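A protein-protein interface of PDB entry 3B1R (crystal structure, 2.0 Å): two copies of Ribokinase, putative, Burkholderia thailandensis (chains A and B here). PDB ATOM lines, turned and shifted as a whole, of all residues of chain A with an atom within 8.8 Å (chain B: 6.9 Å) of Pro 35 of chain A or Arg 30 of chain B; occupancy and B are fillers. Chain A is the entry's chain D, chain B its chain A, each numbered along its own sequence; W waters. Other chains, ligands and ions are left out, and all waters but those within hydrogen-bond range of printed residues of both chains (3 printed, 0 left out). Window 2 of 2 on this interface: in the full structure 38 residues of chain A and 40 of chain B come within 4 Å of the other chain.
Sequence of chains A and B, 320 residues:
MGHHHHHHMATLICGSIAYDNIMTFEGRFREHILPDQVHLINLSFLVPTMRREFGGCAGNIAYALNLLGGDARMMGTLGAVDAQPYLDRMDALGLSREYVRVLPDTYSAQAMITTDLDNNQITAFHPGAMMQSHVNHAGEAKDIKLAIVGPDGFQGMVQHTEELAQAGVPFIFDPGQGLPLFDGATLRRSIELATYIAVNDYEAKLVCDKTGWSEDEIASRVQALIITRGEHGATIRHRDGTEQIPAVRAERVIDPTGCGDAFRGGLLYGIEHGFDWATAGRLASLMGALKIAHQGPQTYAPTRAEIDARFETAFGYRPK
Among the printed residues, merely in contact across the chains: His 39 of chain A with Asn 120 of chain B (3.3 Å), His 39 of chain A with Asp 118 of chain B (3.3 Å), Leu 40 of chain A with Arg 30 of chain B (3.6 Å), Tyr 202 of chain A with Leu 34 of chain B (3.6 Å), Tyr 202 of chain A with Ile 41 of chain B (3.7 Å), Ile 122 of chain A with Phe 29 of chain B (3.8 Å) and Val 38 of chain A with Asp 118 of chain B (3.98 Å).
Water W1 lies within hydrogen-bond range of the side-chain carboxylate (OD2) of Asp 118 of chain B (2.5 Å), the side-chain amide nitrogen (ND2) of Asn 120 of chain B (2.9 Å), the backbone carbonyl oxygen (O) of Val 38 of chain A (3.0 Å) and the backbone NH (N) of Leu 40 of chain A (3.3 Å). Water W3 lies within hydrogen-bond range of the backbone carbonyl oxygen (O) of Val 38 of chain A (3.0 Å) and the side-chain carboxylate (OD2) of Asp 118 of chain B (3.3 Å). Water W2 lies within hydrogen-bond range of the backbone carbonyl oxygen of Asp 118 of chain B (3.0 Å) and a ring nitrogen (NE2) of His 39 of chain A (3.1 Å).
Printed residues of chain B that touch a printed residue of chain A: Phe 29, Arg 30, His 32, Leu 34, Ile 41, Asp 118 and Asn 120. Hydrophobic or aromatic side chains of chain B that line the printed part of chain A: Phe 29, His 32 and Leu 34. Hydrophobic or aromatic side chains of chain A that line the printed part of chain B: Pro 35, His 39, Leu 40, Ile 41, Ile 122 and Tyr 202. Among the printed residues, no Asp or Glu carboxylate lies within 4 Å of a Lys or Arg side-chain nitrogen of the other chain.
6 positions are printed for both chains. Of the 11 pairs that touch across the chains among the printed residues, none has its exchanged pair printed and touching as well.
O of Arg 28 of chain B is in hydrogen-bond range of ND1 of His 32 of chain B (3.1 Å). The guanidinium group (NH1) of Arg 28 of chain B lies within salt-bridge range of the side-chain carboxylate (OD1) of Asp 118 of chain B, 2.8 Å away. The side-chain carboxylate (OD1) of Asp 116 of chain B lies within hydrogen-bond range of the backbone NH (N) of Phe 29 of chain B (2.6 Å). The side-chain carboxylate (OD2) of Asp 116 of chain B lies within hydrogen-bond range of the backbone NH (N) of Asp 118 of chain B. The backbone NH of Asn 120 of chain B lies within hydrogen-bond range of the side-chain carboxylate of Asp 116 of chain B (3.1 Å). The backbone NH (N) of Leu 34 of chain A sits at hydrogen-bond distance from the backbone carbonyl oxygen (O) of Leu 40 of chain A (2.9 Å).
Of chain B, only Arg 30 (2.6 Å) comes within 4 Å of Pro 35 of chain A. Of the printed residues of chain B, Ile 122 of chain A touches Phe 29 (3.8 Å). Of the printed residues of chain A, His 32 of chain B touches Tyr 202. Of the printed residues of chain A, Ile 41 of chain B touches Tyr 202.
NH1 of Arg 30 of chain B lies within hydrogen-bond range of O of Pro 35 of chain A (2.6 Å). O of His 32 of chain B is in hydrogen-bond range of OH of Tyr 202 of chain A. The side-chain amide oxygen (OD1) of Asn 120 of chain B sits at hydrogen-bond distance from the backbone NH (N) of Leu 40 of chain A. The backbone NH of Ile 41 of chain A sits at hydrogen-bond distance from the side-chain amide oxygen of Asn 120 of chain B, at 2.8 Å.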
ATOM      1  N   ARG A  30      13.334  23.127  -2.102  1.00  0.00           N
ATOM      2  CA  ARG A  30      14.097  23.804  -1.052  1.00  0.00           C
ATOM      3  C   ARG A  30      13.357  23.808   0.289  1.00  0.00           C
ATOM      4  O   ARG A  30      13.981  23.842   1.348  1.00  0.00           O
ATOM      5  CB  ARG A  30      14.454  25.234  -1.487  1.00  0.00           C
ATOM      6  CG  ARG A  30      15.403  25.973  -0.563  1.00  0.00           C
ATOM      7  CD  ARG A  30      15.674  27.390  -1.055  1.00  0.00           C
ATOM      8  NE  ARG A  30      16.446  27.417  -2.302  1.00  0.00           N
ATOM      9  CZ  ARG A  30      17.746  27.710  -2.388  1.00  0.00           C
ATOM     10  NH1 ARG A  30      18.450  28.015  -1.305  1.00  0.00           N
ATOM     11  NH2 ARG A  30      18.342  27.720  -3.573  1.00  0.00           N
ATOM     12  N   GLU A  31      12.029  23.745   0.234  1.00  0.00           N
ATOM     13  CA  GLU A  31      11.219  23.724   1.439  1.00  0.00           C
ATOM     14  C   GLU A  31      11.088  22.339   2.071  1.00  0.00           C
ATOM     15  O   GLU A  31      10.724  22.236   3.236  1.00  0.00           O
ATOM     16  CB  GLU A  31       9.844  24.345   1.174  1.00  0.00           C
ATOM     17  CG  GLU A  31       9.850  25.853   1.370  1.00  0.00           C
ATOM     18  CD  GLU A  31       9.172  26.628   0.250  1.00  0.00           C
ATOM     19  OE1 GLU A  31       8.554  26.016  -0.653  1.00  0.00           O
ATOM     20  OE2 GLU A  31       9.264  27.875   0.278  1.00  0.00           O
ATOM     21  N   HIS A  32      11.393  21.280   1.326  1.00  0.00           N
ATOM     22  CA  HIS A  32      11.220  19.927   1.874  1.00  0.00           C
ATOM     23  C   HIS A  32      12.527  19.215   2.211  1.00  0.00           C
ATOM     24  O   HIS A  32      12.531  18.031   2.558  1.00  0.00           O
ATOM     25  CB  HIS A  32      10.310  19.095   0.979  1.00  0.00           C
ATOM     26  CG  HIS A  32       8.979  19.737   0.751  1.00  0.00           C
ATOM     27  ND1 HIS A  32       8.058  19.912   1.761  1.00  0.00           N
ATOM     28  CD2 HIS A  32       8.435  20.293  -0.355  1.00  0.00           C
ATOM     29  CE1 HIS A  32       6.995  20.533   1.282  1.00  0.00           C
ATOM     30  NE2 HIS A  32       7.196  20.770  -0.002  1.00  0.00           N
ATOM     31  N   ILE A  33      13.633  19.945   2.130  1.00  0.00           N
ATOM     32  CA  ILE A  33      14.930  19.368   2.446  1.00  0.00           C
ATOM     33  C   ILE A  33      15.186  19.385   3.946  1.00  0.00           C
ATOM     34  O   ILE A  33      14.891  20.366   4.627  1.00  0.00           O
ATOM     35  CB  ILE A  33      16.060  20.090   1.682  1.00  0.00           C
ATOM     36  CG1 ILE A  33      16.037  19.676   0.207  1.00  0.00           C
ATOM     37  CG2 ILE A  33      17.428  19.800   2.303  1.00  0.00           C
ATOM     38  CD1 ILE A  33      16.675  20.676  -0.681  1.00  0.00           C
ATOM     39  N   LEU A  34      15.716  18.273   4.450  1.00  0.00           N
ATOM     40  CA  LEU A  34      16.120  18.170   5.838  1.00  0.00           C
ATOM     41  C   LEU A  34      17.561  17.684   5.854  1.00  0.00           C
ATOM     42  O   LEU A  34      17.821  16.480   5.749  1.00  0.00           O
ATOM     43  CB  LEU A  34      15.186  17.234   6.623  1.00  0.00           C
ATOM     44  CG  LEU A  34      13.753  17.736   6.863  1.00  0.00           C
ATOM     45  CD1 LEU A  34      12.874  16.660   7.512  1.00  0.00           C
ATOM     46  CD2 LEU A  34      13.726  19.026   7.711  1.00  0.00           C
ATOM     47  N   PRO A  35      18.516  18.630   5.949  1.00  0.00           N
ATOM     48  CA  PRO A  35      19.936  18.266   5.854  1.00  0.00           C
ATOM     49  C   PRO A  35      20.385  17.413   7.030  1.00  0.00           C
ATOM     50  O   PRO A  35      21.200  16.514   6.856  1.00  0.00           O
ATOM     51  CB  PRO A  35      20.656  19.625   5.860  1.00  0.00           C
ATOM     52  CG  PRO A  35      19.579  20.639   5.550  1.00  0.00           C
ATOM     53  CD  PRO A  35      18.338  20.078   6.154  1.00  0.00           C
ATOM     54  N   ASP A  36      19.821  17.683   8.204  1.00  0.00           N
ATOM     55  CA  ASP A  36      20.160  16.977   9.445  1.00  0.00           C
ATOM     56  C   ASP A  36      19.684  15.519   9.478  1.00  0.00           C
ATOM     57  O   ASP A  36      19.746  14.857  10.521  1.00  0.00           O
ATOM     58  CB  ASP A  36      19.617  17.741  10.671  1.00  0.00           C
ATOM     59  CG  ASP A  36      18.075  17.842  10.701  1.00  0.00           C
ATOM     60  OD1 ASP A  36      17.553  18.313  11.736  1.00  0.00           O
ATOM     61  OD2 ASP A  36      17.380  17.472   9.712  1.00  0.00           O
ATOM     62  N   GLN A  37      19.210  15.028   8.339  1.00  0.00           N
ATOM     63  CA  GLN A  37      18.724  13.660   8.224  1.00  0.00           C
ATOM     64  C   GLN A  37      19.531  12.910   7.177  1.00  0.00           C
ATOM     65  O   GLN A  37      20.024  13.521   6.221  1.00  0.00           O
ATOM     66  CB  GLN A  37      17.234  13.651   7.854  1.00  0.00           C
ATOM     67  CG  GLN A  37      16.310  14.283   8.891  1.00  0.00           C
ATOM     68  CD  GLN A  37      16.413  13.626  10.263  1.00  0.00           C
ATOM     69  OE1 GLN A  37      17.047  14.156  11.171  1.00  0.00           O
ATOM     70  NE2 GLN A  37      15.809  12.467  10.408  1.00  0.00           N
ATOM     71  N   VAL A  38      19.671  11.596   7.362  1.00  0.00           N
ATOM     72  CA  VAL A  38      20.335  10.730   6.376  1.00  0.00           C
ATOM     73  C   VAL A  38      19.651  10.835   4.991  1.00  0.00           C
ATOM     74  O   VAL A  38      20.327  10.942   3.969  1.00  0.00           O
ATOM     75  CB  VAL A  38      20.421   9.261   6.884  1.00  0.00           C
ATOM     76  CG1 VAL A  38      20.936   8.314   5.800  1.00  0.00           C
ATOM     77  CG2 VAL A  38      21.304   9.189   8.132  1.00  0.00           C
ATOM     78  N   HIS A  39      18.317  10.824   4.973  1.00  0.00           N
ATOM     79  CA  HIS A  39      17.546  11.075   3.756  1.00  0.00           C
ATOM     80  C   HIS A  39      17.238  12.566   3.640  1.00  0.00           C
ATOM     81  O   HIS A  39      16.501  13.120   4.466  1.00  0.00           O
ATOM     82  CB  HIS A  39      16.233  10.308   3.779  1.00  0.00           C
ATOM     83  CG  HIS A  39      16.401   8.834   3.949  1.00  0.00           C
ATOM     84  ND1 HIS A  39      16.303   8.213   5.177  1.00  0.00           N
ATOM     85  CD2 HIS A  39      16.661   7.858   3.050  1.00  0.00           C
ATOM     86  CE1 HIS A  39      16.491   6.913   5.023  1.00  0.00           C
ATOM     87  NE2 HIS A  39      16.707   6.671   3.742  1.00  0.00           N
ATOM     88  N   LEU A  40      17.803  13.202   2.617  1.00  0.00           N
ATOM     89  CA  LEU A  40      17.676  14.656   2.425  1.00  0.00           C
ATOM     90  C   LEU A  40      16.269  15.114   2.031  1.00  0.00           C
ATOM     91  O   LEU A  40      15.809  16.186   2.447  1.00  0.00           O
ATOM     92  CB  LEU A  40      18.692  15.134   1.373  1.00  0.00           C
ATOM     93  CG  LEU A  40      18.853  16.644   1.153  1.00  0.00           C
ATOM     94  CD1 LEU A  40      19.634  17.242   2.314  1.00  0.00           C
ATOM     95  CD2 LEU A  40      19.574  16.881  -0.159  1.00  0.00           C
ATOM     96  N   ILE A  41      15.590  14.306   1.221  1.00  0.00           N
ATOM     97  CA  ILE A  41      14.284  14.680   0.679  1.00  0.00           C
ATOM     98  C   ILE A  41      13.549  13.426   0.253  1.00  0.00           C
ATOM     99  O   ILE A  41      14.108  12.578  -0.434  1.00  0.00           O
ATOM    100  CB  ILE A  41      14.400  15.739  -0.497  1.00  0.00           C
ATOM    101  CG1 ILE A  41      13.032  16.226  -1.018  1.00  0.00           C
ATOM    102  CG2 ILE A  41      15.417  15.312  -1.577  1.00  0.00           C
ATOM    103  CD1 ILE A  41      12.316  15.337  -2.018  1.00  0.00           C
ATOM    104  N   ILE A 122      15.809  17.863 -12.315  1.00  0.00           N
ATOM    105  CA  ILE A 122      16.534  16.599 -12.177  1.00  0.00           C
ATOM    106  C   ILE A 122      16.019  15.687 -13.287  1.00  0.00           C
ATOM    107  O   ILE A 122      14.855  15.275 -13.292  1.00  0.00           O
ATOM    108  CB  ILE A 122      16.338  15.957 -10.797  1.00  0.00           C
ATOM    109  CG1 ILE A 122      16.686  16.960  -9.687  1.00  0.00           C
ATOM    110  CG2 ILE A 122      17.148  14.648 -10.668  1.00  0.00           C
ATOM    111  CD1 ILE A 122      16.321  16.498  -8.296  1.00  0.00           C
ATOM    112  N   TYR A 202      23.513  28.328 -11.256  1.00  0.00           N
ATOM    113  CA  TYR A 202      24.071  27.037 -10.841  1.00  0.00           C
ATOM    114  C   TYR A 202      25.065  26.525 -11.871  1.00  0.00           C
ATOM    115  O   TYR A 202      26.092  25.948 -11.514  1.00  0.00           O
ATOM    116  CB  TYR A 202      22.938  26.039 -10.691  1.00  0.00           C
ATOM    117  CG  TYR A 202      23.333  24.651 -10.220  1.00  0.00           C
ATOM    118  CD1 TYR A 202      23.764  23.685 -11.122  1.00  0.00           C
ATOM    119  CD2 TYR A 202      23.226  24.300  -8.879  1.00  0.00           C
ATOM    120  CE1 TYR A 202      24.097  22.405 -10.699  1.00  0.00           C
ATOM    121  CE2 TYR A 202      23.558  23.014  -8.439  1.00  0.00           C
ATOM    122  CZ  TYR A 202      23.982  22.074  -9.356  1.00  0.00           C
ATOM    123  OH  TYR A 202      24.318  20.806  -8.952  1.00  0.00           O
ATOM    124  N   GLY B  27      24.829   8.417  -7.811  1.00  0.00           N
ATOM    125  CA  GLY B  27      25.476   9.517  -7.104  1.00  0.00           C
ATOM    126  C   GLY B  27      24.597   9.931  -5.942  1.00  0.00           C
ATOM    127  O   GLY B  27      23.694   9.199  -5.546  1.00  0.00           O
ATOM    128  N   ARG B  28      24.856  11.106  -5.391  1.00  0.00           N
ATOM    129  CA  ARG B  28      24.076  11.577  -4.267  1.00  0.00           C
ATOM    130  C   ARG B  28      23.669  13.015  -4.478  1.00  0.00           C
ATOM    131  O   ARG B  28      24.532  13.885  -4.660  1.00  0.00           O
ATOM    132  CB  ARG B  28      24.840  11.374  -2.958  1.00  0.00           C
ATOM    133  CG  ARG B  28      24.860   9.885  -2.538  1.00  0.00           C
ATOM    134  CD  ARG B  28      26.088   9.511  -1.716  1.00  0.00           C
ATOM    135  NE  ARG B  28      26.584   8.162  -2.049  1.00  0.00           N
ATOM    136  CZ  ARG B  28      26.000   7.020  -1.692  1.00  0.00           C
ATOM    137  NH1 ARG B  28      24.878   7.024  -0.983  1.00  0.00           N
ATOM    138  NH2 ARG B  28      26.539   5.863  -2.047  1.00  0.00           N
ATOM    139  N   PHE B  29      22.351  13.245  -4.476  1.00  0.00           N
ATOM    140  CA  PHE B  29      21.772  14.569  -4.712  1.00  0.00           C
ATOM    141  C   PHE B  29      22.433  15.610  -3.815  1.00  0.00           C
ATOM    142  O   PHE B  29      22.629  16.771  -4.219  1.00  0.00           O
ATOM    143  CB  PHE B  29      20.262  14.569  -4.444  1.00  0.00           C
ATOM    144  CG  PHE B  29      19.439  13.812  -5.464  1.00  0.00           C
ATOM    145  CD1 PHE B  29      19.828  13.732  -6.789  1.00  0.00           C
ATOM    146  CD2 PHE B  29      18.225  13.232  -5.091  1.00  0.00           C
ATOM    147  CE1 PHE B  29      19.045  13.055  -7.726  1.00  0.00           C
ATOM    148  CE2 PHE B  29      17.438  12.547  -6.019  1.00  0.00           C
ATOM    149  CZ  PHE B  29      17.853  12.465  -7.342  1.00  0.00           C
ATOM    150  N   ARG B  30      22.775  15.179  -2.598  1.00  0.00           N
ATOM    151  CA  ARG B  30      23.399  16.028  -1.585  1.00  0.00           C
ATOM    152  C   ARG B  30      24.676  16.729  -2.057  1.00  0.00           C
ATOM    153  O   ARG B  30      24.944  17.878  -1.677  1.00  0.00           O
ATOM    154  CB  ARG B  30      23.708  15.199  -0.344  1.00  0.00           C
ATOM    155  CG  ARG B  30      24.655  15.865   0.641  1.00  0.00           C
ATOM    156  CD  ARG B  30      23.997  17.072   1.309  1.00  0.00           C
ATOM    157  NE  ARG B  30      23.219  16.698   2.487  1.00  0.00           N
ATOM    158  CZ  ARG B  30      23.365  17.255   3.686  1.00  0.00           C
ATOM    159  NH1 ARG B  30      22.610  16.840   4.702  1.00  0.00           N
ATOM    160  NH2 ARG B  30      24.257  18.231   3.866  1.00  0.00           N
ATOM    161  N   GLU B  31      25.470  16.025  -2.859  1.00  0.00           N
ATOM    162  CA  GLU B  31      26.722  16.571  -3.368  1.00  0.00           C
ATOM    163  C   GLU B  31      26.522  17.715  -4.369  1.00  0.00           C
ATOM    164  O   GLU B  31      27.465  18.482  -4.630  1.00  0.00           O
ATOM    165  CB  GLU B  31      27.588  15.458  -3.970  1.00  0.00           C
ATOM    166  CG  GLU B  31      28.300  14.613  -2.906  1.00  0.00           C
ATOM    167  CD  GLU B  31      28.831  13.301  -3.441  1.00  0.00           C
ATOM    168  OE1 GLU B  31      29.275  13.259  -4.609  1.00  0.00           O
ATOM    169  OE2 GLU B  31      28.815  12.307  -2.689  1.00  0.00           O
ATOM    170  N   HIS B  32      25.298  17.845  -4.886  1.00  0.00           N
ATOM    171  CA  HIS B  32      25.002  18.748  -6.000  1.00  0.00           C
ATOM    172  C   HIS B  32      24.002  19.853  -5.661  1.00  0.00           C
ATOM    173  O   HIS B  32      23.470  20.519  -6.547  1.00  0.00           O
ATOM    174  CB  HIS B  32      24.504  17.939  -7.203  1.00  0.00           C
ATOM    175  CG  HIS B  32      25.446  16.862  -7.632  1.00  0.00           C
ATOM    176  ND1 HIS B  32      25.491  15.627  -7.022  1.00  0.00           N
ATOM    177  CD2 HIS B  32      26.388  16.835  -8.606  1.00  0.00           C
ATOM    178  CE1 HIS B  32      26.415  14.884  -7.606  1.00  0.00           C
ATOM    179  NE2 HIS B  32      26.978  15.594  -8.566  1.00  0.00           N
ATOM    180  N   ILE B  33      23.753  20.045  -4.376  1.00  0.00           N
ATOM    181  CA  ILE B  33      22.943  21.154  -3.893  1.00  0.00           C
ATOM    182  C   ILE B  33      23.815  22.416  -3.719  1.00  0.00           C
ATOM    183  O   ILE B  33      24.884  22.353  -3.122  1.00  0.00           O
ATOM    184  CB  ILE B  33      22.241  20.766  -2.551  1.00  0.00           C
ATOM    185  CG1 ILE B  33      21.235  19.619  -2.766  1.00  0.00           C
ATOM    186  CG2 ILE B  33      21.607  21.959  -1.892  1.00  0.00           C
ATOM    187  CD1 ILE B  33      19.866  20.025  -3.317  1.00  0.00           C
ATOM    188  N   LEU B  34      23.360  23.551  -4.261  1.00  0.00           N
ATOM    189  CA  LEU B  34      24.028  24.850  -4.043  1.00  0.00           C
ATOM    190  C   LEU B  34      23.056  25.915  -3.525  1.00  0.00           C
ATOM    191  O   LEU B  34      22.510  26.695  -4.304  1.00  0.00           O
ATOM    192  CB  LEU B  34      24.742  25.343  -5.321  1.00  0.00           C
ATOM    193  CG  LEU B  34      26.188  24.929  -5.670  1.00  0.00           C
ATOM    194  CD1 LEU B  34      27.166  25.220  -4.536  1.00  0.00           C
ATOM    195  CD2 LEU B  34      26.305  23.475  -6.085  1.00  0.00           C
ATOM    196  N   ILE B  41      19.551  22.928  -7.327  1.00  0.00           N
ATOM    197  CA  ILE B  41      20.148  21.749  -7.982  1.00  0.00           C
ATOM    198  C   ILE B  41      19.619  21.601  -9.418  1.00  0.00           C
ATOM    199  O   ILE B  41      18.421  21.725  -9.659  1.00  0.00           O
ATOM    200  CB  ILE B  41      19.890  20.437  -7.165  1.00  0.00           C
ATOM    201  CG1 ILE B  41      20.449  19.193  -7.886  1.00  0.00           C
ATOM    202  CG2 ILE B  41      18.397  20.257  -6.841  1.00  0.00           C
ATOM    203  CD1 ILE B  41      20.673  18.001  -6.956  1.00  0.00           C
ATOM    204  N   ASP B 116      18.292   8.887  -5.924  1.00  0.00           N
ATOM    205  CA  ASP B 116      19.746   8.757  -5.928  1.00  0.00           C
ATOM    206  C   ASP B 116      20.167   7.578  -5.036  1.00  0.00           C
ATOM    207  O   ASP B 116      19.321   6.791  -4.612  1.00  0.00           O
ATOM    208  CB  ASP B 116      20.409  10.064  -5.489  1.00  0.00           C
ATOM    209  CG  ASP B 116      20.212  10.371  -4.010  1.00  0.00           C
ATOM    210  OD1 ASP B 116      20.789  11.379  -3.560  1.00  0.00           O
ATOM    211  OD2 ASP B 116      19.493   9.627  -3.296  1.00  0.00           O
ATOM    212  N   ASP B 118      21.241   7.757  -2.080  1.00  0.00           N
ATOM    213  CA  ASP B 118      20.840   8.076  -0.709  1.00  0.00           C
ATOM    214  C   ASP B 118      19.369   7.785  -0.468  1.00  0.00           C
ATOM    215  O   ASP B 118      18.836   8.144   0.588  1.00  0.00           O
ATOM    216  CB  ASP B 118      21.080   9.559  -0.404  1.00  0.00           C
ATOM    217  CG  ASP B 118      22.410   9.809   0.254  1.00  0.00           C
ATOM    218  OD1 ASP B 118      23.231   8.879   0.284  1.00  0.00           O
ATOM    219  OD2 ASP B 118      22.632  10.943   0.730  1.00  0.00           O
ATOM    220  N   ASN B 120      16.832   9.240  -1.731  1.00  0.00           N
ATOM    221  CA  ASN B 120      16.021  10.440  -1.823  1.00  0.00           C
ATOM    222  C   ASN B 120      15.003  10.323  -2.975  1.00  0.00           C
ATOM    223  O   ASN B 120      15.172  10.925  -4.053  1.00  0.00           O
ATOM    224  CB  ASN B 120      16.910  11.690  -1.969  1.00  0.00           C
ATOM    225  CG  ASN B 120      17.682  12.013  -0.694  1.00  0.00           C
ATOM    226  OD1 ASN B 120      17.109  12.097   0.389  1.00  0.00           O
ATOM    227  ND2 ASN B 120      18.988  12.212  -0.825  1.00  0.00           N
HETATM  228  O   HOH W   1      20.827  12.562   1.442  1.00  0.00           O
HETATM  229  O   HOH W   2      19.721   6.513   2.964  1.00  0.00           O
HETATM  230  O   HOH W   3      23.336  11.043   3.959  1.00  0.00           O
